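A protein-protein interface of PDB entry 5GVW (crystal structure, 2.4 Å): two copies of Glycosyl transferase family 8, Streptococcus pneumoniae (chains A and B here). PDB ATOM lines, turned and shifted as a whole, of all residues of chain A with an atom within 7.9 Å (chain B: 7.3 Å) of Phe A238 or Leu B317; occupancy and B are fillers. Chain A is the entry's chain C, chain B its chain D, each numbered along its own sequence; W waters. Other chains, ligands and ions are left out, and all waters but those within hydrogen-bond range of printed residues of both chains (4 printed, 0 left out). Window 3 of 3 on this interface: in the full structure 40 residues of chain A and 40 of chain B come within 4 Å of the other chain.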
ATOM      1  N   GLN A 231      12.450  19.816  41.147  1.00  0.00           N
ATOM      2  CA  GLN A 231      12.806  19.635  39.725  1.00  0.00           C
ATOM      3  C   GLN A 231      11.763  20.120  38.678  1.00  0.00           C
ATOM      4  O   GLN A 231      12.110  20.377  37.525  1.00  0.00           O
ATOM      5  CB  GLN A 231      13.157  18.169  39.471  1.00  0.00           C
ATOM      6  CG  GLN A 231      14.450  17.763  40.175  1.00  0.00           C
ATOM      7  CD  GLN A 231      14.875  16.323  39.881  1.00  0.00           C
ATOM      8  OE1 GLN A 231      14.115  15.542  39.285  1.00  0.00           O
ATOM      9  NE2 GLN A 231      16.093  15.964  40.302  1.00  0.00           N
ATOM     10  N   ASP A 232      10.509  20.257  39.091  1.00  0.00           N
ATOM     11  CA  ASP A 232       9.451  20.810  38.261  1.00  0.00           C
ATOM     12  C   ASP A 232       9.512  22.331  38.189  1.00  0.00           C
ATOM     13  O   ASP A 232       8.855  23.043  38.951  1.00  0.00           O
ATOM     14  CB  ASP A 232       8.116  20.361  38.830  1.00  0.00           C
ATOM     15  CG  ASP A 232       6.975  20.642  37.920  1.00  0.00           C
ATOM     16  OD1 ASP A 232       7.060  20.180  36.760  1.00  0.00           O
ATOM     17  OD2 ASP A 232       5.988  21.279  38.366  1.00  0.00           O
ATOM     18  N   LYS A 233      10.314  22.836  37.275  1.00  0.00           N
ATOM     19  CA  LYS A 233      10.508  24.273  37.165  1.00  0.00           C
ATOM     20  C   LYS A 233       9.610  24.885  36.095  1.00  0.00           C
ATOM     21  O   LYS A 233       9.452  24.313  35.044  1.00  0.00           O
ATOM     22  CB  LYS A 233      11.966  24.569  36.832  1.00  0.00           C
ATOM     23  CG  LYS A 233      12.973  24.009  37.844  1.00  0.00           C
ATOM     24  CD  LYS A 233      12.827  24.661  39.220  1.00  0.00           C
ATOM     25  CE  LYS A 233      14.087  24.553  40.062  1.00  0.00           C
ATOM     26  NZ  LYS A 233      13.756  24.613  41.509  1.00  0.00           N
ATOM     27  N   PRO A 234       9.072  26.090  36.339  1.00  0.00           N
ATOM     28  CA  PRO A 234       8.257  26.738  35.323  1.00  0.00           C
ATOM     29  C   PRO A 234       9.014  27.120  34.017  1.00  0.00           C
ATOM     30  O   PRO A 234       8.400  27.244  32.932  1.00  0.00           O
ATOM     31  CB  PRO A 234       7.747  27.988  36.054  1.00  0.00           C
ATOM     32  CG  PRO A 234       8.851  28.324  36.996  1.00  0.00           C
ATOM     33  CD  PRO A 234       9.292  26.984  37.502  1.00  0.00           C
ATOM     34  N   TRP A 235      10.321  27.312  34.122  1.00  0.00           N
ATOM     35  CA  TRP A 235      11.144  27.630  32.941  1.00  0.00           C
ATOM     36  C   TRP A 235      11.575  26.418  32.090  1.00  0.00           C
ATOM     37  O   TRP A 235      12.149  26.612  31.042  1.00  0.00           O
ATOM     38  CB  TRP A 235      12.376  28.469  33.336  1.00  0.00           C
ATOM     39  CG  TRP A 235      13.317  27.761  34.225  1.00  0.00           C
ATOM     40  CD1 TRP A 235      14.186  26.785  33.874  1.00  0.00           C
ATOM     41  CD2 TRP A 235      13.458  27.944  35.635  1.00  0.00           C
ATOM     42  NE1 TRP A 235      14.873  26.340  34.977  1.00  0.00           N
ATOM     43  CE2 TRP A 235      14.452  27.044  36.074  1.00  0.00           C
ATOM     44  CE3 TRP A 235      12.843  28.786  36.570  1.00  0.00           C
ATOM     45  CZ2 TRP A 235      14.847  26.952  37.407  1.00  0.00           C
ATOM     46  CZ3 TRP A 235      13.246  28.703  37.906  1.00  0.00           C
ATOM     47  CH2 TRP A 235      14.228  27.781  38.307  1.00  0.00           C
ATOM     48  N   ASN A 236      11.322  25.193  32.534  1.00  0.00           N
ATOM     49  CA  ASN A 236      11.497  24.022  31.655  1.00  0.00           C
ATOM     50  C   ASN A 236      10.470  23.973  30.551  1.00  0.00           C
ATOM     51  O   ASN A 236       9.415  24.576  30.652  1.00  0.00           O
ATOM     52  CB  ASN A 236      11.441  22.701  32.432  1.00  0.00           C
ATOM     53  CG  ASN A 236      12.535  22.604  33.443  1.00  0.00           C
ATOM     54  OD1 ASN A 236      13.608  23.173  33.247  1.00  0.00           O
ATOM     55  ND2 ASN A 236      12.283  21.905  34.536  1.00  0.00           N
ATOM     56  N   GLN A 237      10.793  23.214  29.512  1.00  0.00           N
ATOM     57  CA  GLN A 237       9.915  23.041  28.354  1.00  0.00           C
ATOM     58  C   GLN A 237       8.538  22.592  28.825  1.00  0.00           C
ATOM     59  O   GLN A 237       7.516  23.134  28.392  1.00  0.00           O
ATOM     60  CB  GLN A 237      10.496  21.997  27.380  1.00  0.00           C
ATOM     61  CG  GLN A 237       9.695  21.863  26.086  1.00  0.00           C
ATOM     62  CD  GLN A 237      10.240  20.810  25.133  1.00  0.00           C
ATOM     63  OE1 GLN A 237      10.981  19.887  25.525  1.00  0.00           O
ATOM     64  NE2 GLN A 237       9.875  20.943  23.862  1.00  0.00           N
ATOM     65  N   PHE A 238       8.547  21.598  29.712  1.00  0.00           N
ATOM     66  CA  PHE A 238       7.343  21.071  30.338  1.00  0.00           C
ATOM     67  C   PHE A 238       7.399  21.231  31.856  1.00  0.00           C
ATOM     68  O   PHE A 238       8.429  20.989  32.477  1.00  0.00           O
ATOM     69  CB  PHE A 238       7.199  19.587  30.001  1.00  0.00           C
ATOM     70  CG  PHE A 238       7.266  19.293  28.540  1.00  0.00           C
ATOM     71  CD1 PHE A 238       6.382  19.913  27.651  1.00  0.00           C
ATOM     72  CD2 PHE A 238       8.204  18.392  28.046  1.00  0.00           C
ATOM     73  CE1 PHE A 238       6.450  19.649  26.290  1.00  0.00           C
ATOM     74  CE2 PHE A 238       8.266  18.118  26.685  1.00  0.00           C
ATOM     75  CZ  PHE A 238       7.388  18.742  25.809  1.00  0.00           C
ATOM     76  N   SER A 239       6.289  21.640  32.454  1.00  0.00           N
ATOM     77  CA  SER A 239       6.105  21.486  33.901  1.00  0.00           C
ATOM     78  C   SER A 239       4.638  21.366  34.209  1.00  0.00           C
ATOM     79  O   SER A 239       3.783  21.886  33.495  1.00  0.00           O
ATOM     80  CB  SER A 239       6.641  22.673  34.656  1.00  0.00           C
ATOM     81  OG  SER A 239       5.947  23.868  34.269  1.00  0.00           O
ATOM     82  N   VAL A 240       4.382  20.743  35.333  1.00  0.00           N
ATOM     83  CA  VAL A 240       3.033  20.436  35.807  1.00  0.00           C
ATOM     84  C   VAL A 240       2.475  21.416  36.850  1.00  0.00           C
ATOM     85  O   VAL A 240       1.254  21.529  37.022  1.00  0.00           O
ATOM     86  CB  VAL A 240       3.023  19.009  36.361  1.00  0.00           C
ATOM     87  CG1 VAL A 240       3.363  18.042  35.231  1.00  0.00           C
ATOM     88  CG2 VAL A 240       4.002  18.826  37.521  1.00  0.00           C
ATOM     89  N   GLY A 241       3.375  22.113  37.544  1.00  0.00           N
ATOM     90  CA  GLY A 241       3.010  23.019  38.610  1.00  0.00           C
ATOM     91  C   GLY A 241       2.230  24.226  38.122  1.00  0.00           C
ATOM     92  O   GLY A 241       2.293  24.585  36.949  1.00  0.00           O
ATOM     93  N   ARG A 244       2.905  28.825  36.350  1.00  0.00           N
ATOM     94  CA  ARG A 244       3.967  28.780  35.339  1.00  0.00           C
ATOM     95  C   ARG A 244       3.997  30.099  34.612  1.00  0.00           C
ATOM     96  O   ARG A 244       5.031  30.699  34.492  1.00  0.00           O
ATOM     97  CB  ARG A 244       3.694  27.643  34.366  1.00  0.00           C
ATOM     98  CG  ARG A 244       4.860  27.244  33.521  1.00  0.00           C
ATOM     99  CD  ARG A 244       4.431  26.445  32.306  1.00  0.00           C
ATOM    100  NE  ARG A 244       5.292  26.687  31.138  1.00  0.00           N
ATOM    101  CZ  ARG A 244       6.381  25.997  30.805  1.00  0.00           C
ATOM    102  NH1 ARG A 244       6.826  24.983  31.538  1.00  0.00           N
ATOM    103  NH2 ARG A 244       7.040  26.331  29.714  1.00  0.00           N
ATOM    104  N   GLN B  41      14.474  21.852  19.440  1.00  0.00           N
ATOM    105  CA  GLN B  41      13.871  20.651  20.023  1.00  0.00           C
ATOM    106  C   GLN B  41      13.080  20.921  21.325  1.00  0.00           C
ATOM    107  O   GLN B  41      11.968  20.352  21.533  1.00  0.00           O
ATOM    108  CB  GLN B  41      15.006  19.689  20.299  1.00  0.00           C
ATOM    109  CG  GLN B  41      14.612  18.323  20.793  1.00  0.00           C
ATOM    110  CD  GLN B  41      15.822  17.411  20.920  1.00  0.00           C
ATOM    111  OE1 GLN B  41      16.984  17.843  20.773  1.00  0.00           O
ATOM    112  NE2 GLN B  41      15.560  16.140  21.212  1.00  0.00           N
ATOM    113  N   ASP B  42      13.665  21.780  22.178  1.00  0.00           N
ATOM    114  CA  ASP B  42      13.207  22.000  23.556  1.00  0.00           C
ATOM    115  C   ASP B  42      12.925  23.456  23.978  1.00  0.00           C
ATOM    116  O   ASP B  42      12.623  23.712  25.128  1.00  0.00           O
ATOM    117  CB  ASP B  42      14.146  21.291  24.568  1.00  0.00           C
ATOM    118  CG  ASP B  42      15.614  21.717  24.449  1.00  0.00           C
ATOM    119  OD1 ASP B  42      15.880  22.788  23.829  1.00  0.00           O
ATOM    120  OD2 ASP B  42      16.494  20.951  24.969  1.00  0.00           O
ATOM    121  N   PRO B  44      10.993  26.352  25.162  1.00  0.00           N
ATOM    122  CA  PRO B  44       9.609  26.573  25.631  1.00  0.00           C
ATOM    123  C   PRO B  44       8.809  27.564  24.777  1.00  0.00           C
ATOM    124  O   PRO B  44       9.391  28.439  24.121  1.00  0.00           O
ATOM    125  CB  PRO B  44       9.785  27.167  27.043  1.00  0.00           C
ATOM    126  CG  PRO B  44      11.205  26.959  27.412  1.00  0.00           C
ATOM    127  CD  PRO B  44      11.993  26.753  26.174  1.00  0.00           C
ATOM    128  N   GLN B  45       7.483  27.409  24.837  1.00  0.00           N
ATOM    129  CA  GLN B  45       6.542  28.092  23.947  1.00  0.00           C
ATOM    130  C   GLN B  45       6.229  29.514  24.343  1.00  0.00           C
ATOM    131  O   GLN B  45       5.831  30.306  23.471  1.00  0.00           O
ATOM    132  CB  GLN B  45       5.222  27.338  23.896  1.00  0.00           C
ATOM    133  CG  GLN B  45       5.343  25.961  23.298  1.00  0.00           C
ATOM    134  CD  GLN B  45       4.156  25.097  23.662  1.00  0.00           C
ATOM    135  OE1 GLN B  45       4.036  24.618  24.802  1.00  0.00           O
ATOM    136  NE2 GLN B  45       3.258  24.898  22.699  1.00  0.00           N
ATOM    137  N   LYS B  66       9.756  22.697  15.324  1.00  0.00           N
ATOM    138  CA  LYS B  66      10.116  21.586  16.229  1.00  0.00           C
ATOM    139  C   LYS B  66      10.704  20.313  15.565  1.00  0.00           C
ATOM    140  O   LYS B  66      10.046  19.636  14.798  1.00  0.00           O
ATOM    141  CB  LYS B  66       8.945  21.256  17.164  1.00  0.00           C
ATOM    142  CG  LYS B  66       8.752  22.280  18.299  1.00  0.00           C
ATOM    143  CD  LYS B  66       9.935  22.280  19.285  1.00  0.00           C
ATOM    144  CE  LYS B  66       9.654  23.000  20.592  1.00  0.00           C
ATOM    145  NZ  LYS B  66       9.402  24.461  20.392  1.00  0.00           N
ATOM    146  N   ILE B  68      11.079  17.226  16.549  1.00  0.00           N
ATOM    147  CA  ILE B  68      10.560  16.187  17.443  1.00  0.00           C
ATOM    148  C   ILE B  68       9.961  15.102  16.531  1.00  0.00           C
ATOM    149  O   ILE B  68       9.064  15.376  15.722  1.00  0.00           O
ATOM    150  CB  ILE B  68       9.490  16.778  18.421  1.00  0.00           C
ATOM    151  CG1 ILE B  68      10.117  17.810  19.352  1.00  0.00           C
ATOM    152  CG2 ILE B  68       8.872  15.700  19.314  1.00  0.00           C
ATOM    153  CD1 ILE B  68       9.134  18.735  20.028  1.00  0.00           C
ATOM    154  N   ASN B 311       5.239   9.515  30.484  1.00  0.00           N
ATOM    155  CA  ASN B 311       5.960  10.097  29.358  1.00  0.00           C
ATOM    156  C   ASN B 311       5.069  10.142  28.123  1.00  0.00           C
ATOM    157  O   ASN B 311       4.232   9.269  27.963  1.00  0.00           O
ATOM    158  CB  ASN B 311       7.197   9.247  29.090  1.00  0.00           C
ATOM    159  CG  ASN B 311       8.179   9.292  30.238  1.00  0.00           C
ATOM    160  OD1 ASN B 311       8.319   8.337  31.003  1.00  0.00           O
ATOM    161  ND2 ASN B 311       8.825  10.428  30.398  1.00  0.00           N
ATOM    162  N   MET B 312       5.237  11.137  27.255  1.00  0.00           N
ATOM    163  CA  MET B 312       4.421  11.241  26.018  1.00  0.00           C
ATOM    164  C   MET B 312       5.198  10.839  24.782  1.00  0.00           C
ATOM    165  O   MET B 312       6.423  11.003  24.715  1.00  0.00           O
ATOM    166  CB  MET B 312       3.879  12.655  25.791  1.00  0.00           C
ATOM    167  CG  MET B 312       3.383  13.308  27.051  1.00  0.00           C
ATOM    168  SD  MET B 312       1.677  13.794  27.067  1.00  0.00           S
ATOM    169  CE  MET B 312       1.845  15.467  26.509  1.00  0.00           C
ATOM    170  N   ALA B 313       4.482  10.322  23.793  1.00  0.00           N
ATOM    171  CA  ALA B 313       5.115   9.973  22.536  1.00  0.00           C
ATOM    172  C   ALA B 313       5.292  11.231  21.694  1.00  0.00           C
ATOM    173  O   ALA B 313       4.675  12.281  21.963  1.00  0.00           O
ATOM    174  CB  ALA B 313       4.301   8.934  21.801  1.00  0.00           C
ATOM    175  N   ASN B 314       6.139  11.126  20.675  1.00  0.00           N
ATOM    176  CA  ASN B 314       6.512  12.310  19.889  1.00  0.00           C
ATOM    177  C   ASN B 314       5.343  13.015  19.198  1.00  0.00           C
ATOM    178  O   ASN B 314       5.352  14.242  19.055  1.00  0.00           O
ATOM    179  CB  ASN B 314       7.595  11.972  18.865  1.00  0.00           C
ATOM    180  CG  ASN B 314       8.889  11.531  19.513  1.00  0.00           C
ATOM    181  OD1 ASN B 314       9.253  12.004  20.600  1.00  0.00           O
ATOM    182  ND2 ASN B 314       9.596  10.607  18.858  1.00  0.00           N
ATOM    183  N   GLU B 315       4.339  12.244  18.781  1.00  0.00           N
ATOM    184  CA  GLU B 315       3.156  12.803  18.097  1.00  0.00           C
ATOM    185  C   GLU B 315       2.436  13.845  18.949  1.00  0.00           C
ATOM    186  O   GLU B 315       1.923  14.819  18.400  1.00  0.00           O
ATOM    187  CB  GLU B 315       2.188  11.698  17.628  1.00  0.00           C
ATOM    188  CG  GLU B 315       2.743  10.796  16.507  1.00  0.00           C
ATOM    189  CD  GLU B 315       3.408   9.509  17.007  1.00  0.00           C
ATOM    190  OE1 GLU B 315       3.536   8.549  16.217  1.00  0.00           O
ATOM    191  OE2 GLU B 315       3.797   9.440  18.189  1.00  0.00           O
ATOM    192  N   LEU B 316       2.448  13.659  20.278  1.00  0.00           N
ATOM    193  CA  LEU B 316       1.898  14.638  21.237  1.00  0.00           C
ATOM    194  C   LEU B 316       2.906  15.705  21.673  1.00  0.00           C
ATOM    195  O   LEU B 316       2.553  16.899  21.751  1.00  0.00           O
ATOM    196  CB  LEU B 316       1.381  13.933  22.476  1.00  0.00           C
ATOM    197  CG  LEU B 316       0.178  13.020  22.258  1.00  0.00           C
ATOM    198  CD1 LEU B 316       0.038  12.105  23.457  1.00  0.00           C
ATOM    199  CD2 LEU B 316      -1.104  13.823  22.050  1.00  0.00           C
ATOM    200  N   LEU B 317       4.145  15.288  21.970  1.00  0.00           N
ATOM    201  CA  LEU B 317       5.205  16.244  22.372  1.00  0.00           C
ATOM    202  C   LEU B 317       5.412  17.304  21.295  1.00  0.00           C
ATOM    203  O   LEU B 317       5.650  18.458  21.610  1.00  0.00           O
ATOM    204  CB  LEU B 317       6.550  15.554  22.636  1.00  0.00           C
ATOM    205  CG  LEU B 317       6.738  14.594  23.800  1.00  0.00           C
ATOM    206  CD1 LEU B 317       8.163  14.091  23.782  1.00  0.00           C
ATOM    207  CD2 LEU B 317       6.466  15.237  25.142  1.00  0.00           C
ATOM    208  N   ALA B 318       5.276  16.907  20.033  1.00  0.00           N
ATOM    209  CA  ALA B 318       5.389  17.817  18.919  1.00  0.00           C
ATOM    210  C   ALA B 318       4.299  18.904  18.818  1.00  0.00           C
ATOM    211  O   ALA B 318       4.414  19.810  17.960  1.00  0.00           O
ATOM    212  CB  ALA B 318       5.448  17.033  17.625  1.00  0.00           C
ATOM    213  N   LEU B 319       3.256  18.814  19.658  1.00  0.00           N
ATOM    214  CA  LEU B 319       2.186  19.804  19.675  1.00  0.00           C
ATOM    215  C   LEU B 319       2.682  21.112  20.232  1.00  0.00           C
ATOM    216  O   LEU B 319       2.014  22.136  20.022  1.00  0.00           O
ATOM    217  CB  LEU B 319       0.979  19.326  20.478  1.00  0.00           C
ATOM    218  CG  LEU B 319       0.225  18.089  19.956  1.00  0.00           C
ATOM    219  CD1 LEU B 319      -0.667  17.501  21.032  1.00  0.00           C
ATOM    220  CD2 LEU B 319      -0.609  18.437  18.726  1.00  0.00           C
ATOM    221  N   THR B 320       3.836  21.090  20.931  1.00  0.00           N
ATOM    222  CA  THR B 320       4.575  22.319  21.297  1.00  0.00           C
ATOM    223  C   THR B 320       4.768  23.314  20.144  1.00  0.00           C
ATOM    224  O   THR B 320       4.836  24.528  20.360  1.00  0.00           O
ATOM    225  CB  THR B 320       5.967  22.019  21.859  1.00  0.00           C
ATOM    226  OG1 THR B 320       6.678  21.138  20.974  1.00  0.00           O
ATOM    227  CG2 THR B 320       5.855  21.409  23.261  1.00  0.00           C
ATOM    228  N   ARG B 321       4.826  22.799  18.923  1.00  0.00           N
ATOM    229  CA  ARG B 321       4.855  23.662  17.723  1.00  0.00           C
ATOM    230  C   ARG B 321       3.696  24.675  17.584  1.00  0.00           C
ATOM    231  O   ARG B 321       3.847  25.706  16.930  1.00  0.00           O
ATOM    232  CB  ARG B 321       4.968  22.814  16.446  1.00  0.00           C
ATOM    233  CG  ARG B 321       3.668  22.264  15.891  1.00  0.00           C
ATOM    234  CD  ARG B 321       3.954  21.479  14.629  1.00  0.00           C
ATOM    235  NE  ARG B 321       2.743  20.886  14.098  1.00  0.00           N
ATOM    236  CZ  ARG B 321       2.189  19.781  14.549  1.00  0.00           C
ATOM    237  NH1 ARG B 321       2.720  19.115  15.568  1.00  0.00           N
ATOM    238  NH2 ARG B 321       1.082  19.343  13.980  1.00  0.00           N
ATOM    239  N   THR B 326      -0.909  23.470  25.327  1.00  0.00           N
ATOM    240  CA  THR B 326      -0.002  23.107  26.413  1.00  0.00           C
ATOM    241  C   THR B 326      -0.130  21.639  26.634  1.00  0.00           C
ATOM    242  O   THR B 326      -1.212  21.116  26.687  1.00  0.00           O
ATOM    243  CB  THR B 326      -0.224  23.916  27.714  1.00  0.00           C
ATOM    244  OG1 THR B 326      -0.124  25.322  27.407  1.00  0.00           O
ATOM    245  CG2 THR B 326       0.825  23.580  28.765  1.00  0.00           C
ATOM    246  N   VAL B 327       1.007  20.993  26.801  1.00  0.00           N
ATOM    247  CA  VAL B 327       1.125  19.545  26.932  1.00  0.00           C
ATOM    248  C   VAL B 327       1.743  19.277  28.327  1.00  0.00           C
ATOM    249  O   VAL B 327       2.597  20.038  28.783  1.00  0.00           O
ATOM    250  CB  VAL B 327       1.924  19.027  25.696  1.00  0.00           C
ATOM    251  CG1 VAL B 327       3.286  18.456  26.040  1.00  0.00           C
ATOM    252  CG2 VAL B 327       1.074  18.118  24.804  1.00  0.00           C
ATOM    253  N   TYR B 328       1.268  18.248  29.025  1.00  0.00           N
ATOM    254  CA  TYR B 328       1.673  17.998  30.403  1.00  0.00           C
ATOM    255  C   TYR B 328       2.020  16.525  30.580  1.00  0.00           C
ATOM    256  O   TYR B 328       1.204  15.737  31.075  1.00  0.00           O
ATOM    257  CB  TYR B 328       0.572  18.405  31.407  1.00  0.00           C
ATOM    258  CG  TYR B 328       0.005  19.826  31.311  1.00  0.00           C
ATOM    259  CD1 TYR B 328      -0.911  20.143  30.339  1.00  0.00           C
ATOM    260  CD2 TYR B 328       0.332  20.807  32.240  1.00  0.00           C
ATOM    261  CE1 TYR B 328      -1.481  21.404  30.254  1.00  0.00           C
ATOM    262  CE2 TYR B 328      -0.219  22.078  32.168  1.00  0.00           C
ATOM    263  CZ  TYR B 328      -1.138  22.379  31.168  1.00  0.00           C
ATOM    264  OH  TYR B 328      -1.732  23.636  31.024  1.00  0.00           O
ATOM    265  N   PRO B 329       3.243  16.136  30.196  1.00  0.00           N
ATOM    266  CA  PRO B 329       3.684  14.789  30.550  1.00  0.00           C
ATOM    267  C   PRO B 329       3.910  14.689  32.067  1.00  0.00           C
ATOM    268  O   PRO B 329       4.158  15.704  32.716  1.00  0.00           O
ATOM    269  CB  PRO B 329       5.015  14.633  29.789  1.00  0.00           C
ATOM    270  CG  PRO B 329       5.536  16.007  29.713  1.00  0.00           C
ATOM    271  CD  PRO B 329       4.325  16.904  29.553  1.00  0.00           C
HETATM  272  O   HOH W   1       8.514  23.351  23.461  1.00  0.00           O
HETATM  273  O   HOH W   2       6.629  24.365  25.846  1.00  0.00           O
HETATM  274  O   HOH W   3      11.648  17.748  23.785  1.00  0.00           O
HETATM  275  O   HOH W   4       3.804  21.848  30.525  1.00  0.00           O
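The backbone carbonyl oxygen of Pro A234 lies within hydrogen-bond range of the guanidinium group of Arg A244 (3.1 Å).
O of Asn A236 lies within hydrogen-bond range of NH1 of Arg A244 (2.8 Å).
O of Leu B317 sits at hydrogen-bond distance from OG1 of Thr B320 (2.9 Å).
The guanidinium group (NH1) of Arg A244 is in hydrogen-bond range of the side-chain hydroxyl (OG) of Ser A239, 3.1 Å away.
The side-chain carboxylate of Asp A232 sits at hydrogen-bond distance from the backbone NH of Val A240, 3.1 Å away.
O of Thr B320 lies within hydrogen-bond range of NE2 of Gln B45 (2.8 Å).
The backbone carbonyl oxygen of Gln B41 is in hydrogen-bond range of the side-chain amide nitrogen of Gln A237, at 3.2 Å.
No position is printed for both chains.
Water W4 bridges the backbone carbonyl oxygen (O) of Val B327 (2.8 Å) and the backbone carbonyl oxygen (O) of Ser A239 (3.0 Å).
Water W1 lies within hydrogen-bond range of the side-chain amide nitrogen (NE2) of Gln A237 and the side-chain amino group (NZ) of Lys B66.
Water W2 lies within hydrogen-bond range of OE1 of Gln B45 and O of Gln A237.
Water W3 lies within hydrogen-bond range of OE1 of Gln A237 (2.8 Å) and O of Gln B41 (3.5 Å).
Of chain B, only Leu B317 (3.7 Å), Thr B320 (3.6 Å), Val B327 (3.4 Å) and Pro B329 (3.9 Å) come within 4 Å of Phe A238.
Printed residues of chain B within 4 Å of Trp A235: Pro B44.
Printed residues of chain A within 4 Å of Tyr B328: Ser A239 (3.8 Å).
Of the 12 printed residues of chain A, 6 touch a printed residue of chain B.
Trp A235 touches Pro B44 (O to CG, 3.8 Å).
CA of Asp B42 touches NE2 of Gln A237 (3.5 Å).
Gln A237 touches Lys B66 (NE2 to CE, 3.9 Å).
Leu B317 touches Phe A238.
CE1 of Phe A238 touches CG2 of Thr B320, 3.6 Å away.
Val B327 touches Phe A238 (CG1 to CE1, 3.4 Å).
CG of Phe A238 touches CG of Pro B329, at 3.9 Å.
Tyr B328 touches Ser A239.
CG1 of Val A240 touches O of Pro B329 (3.5 Å).
Arg A244 touches Pro B44 (NH2 to CB, 3.9 Å).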
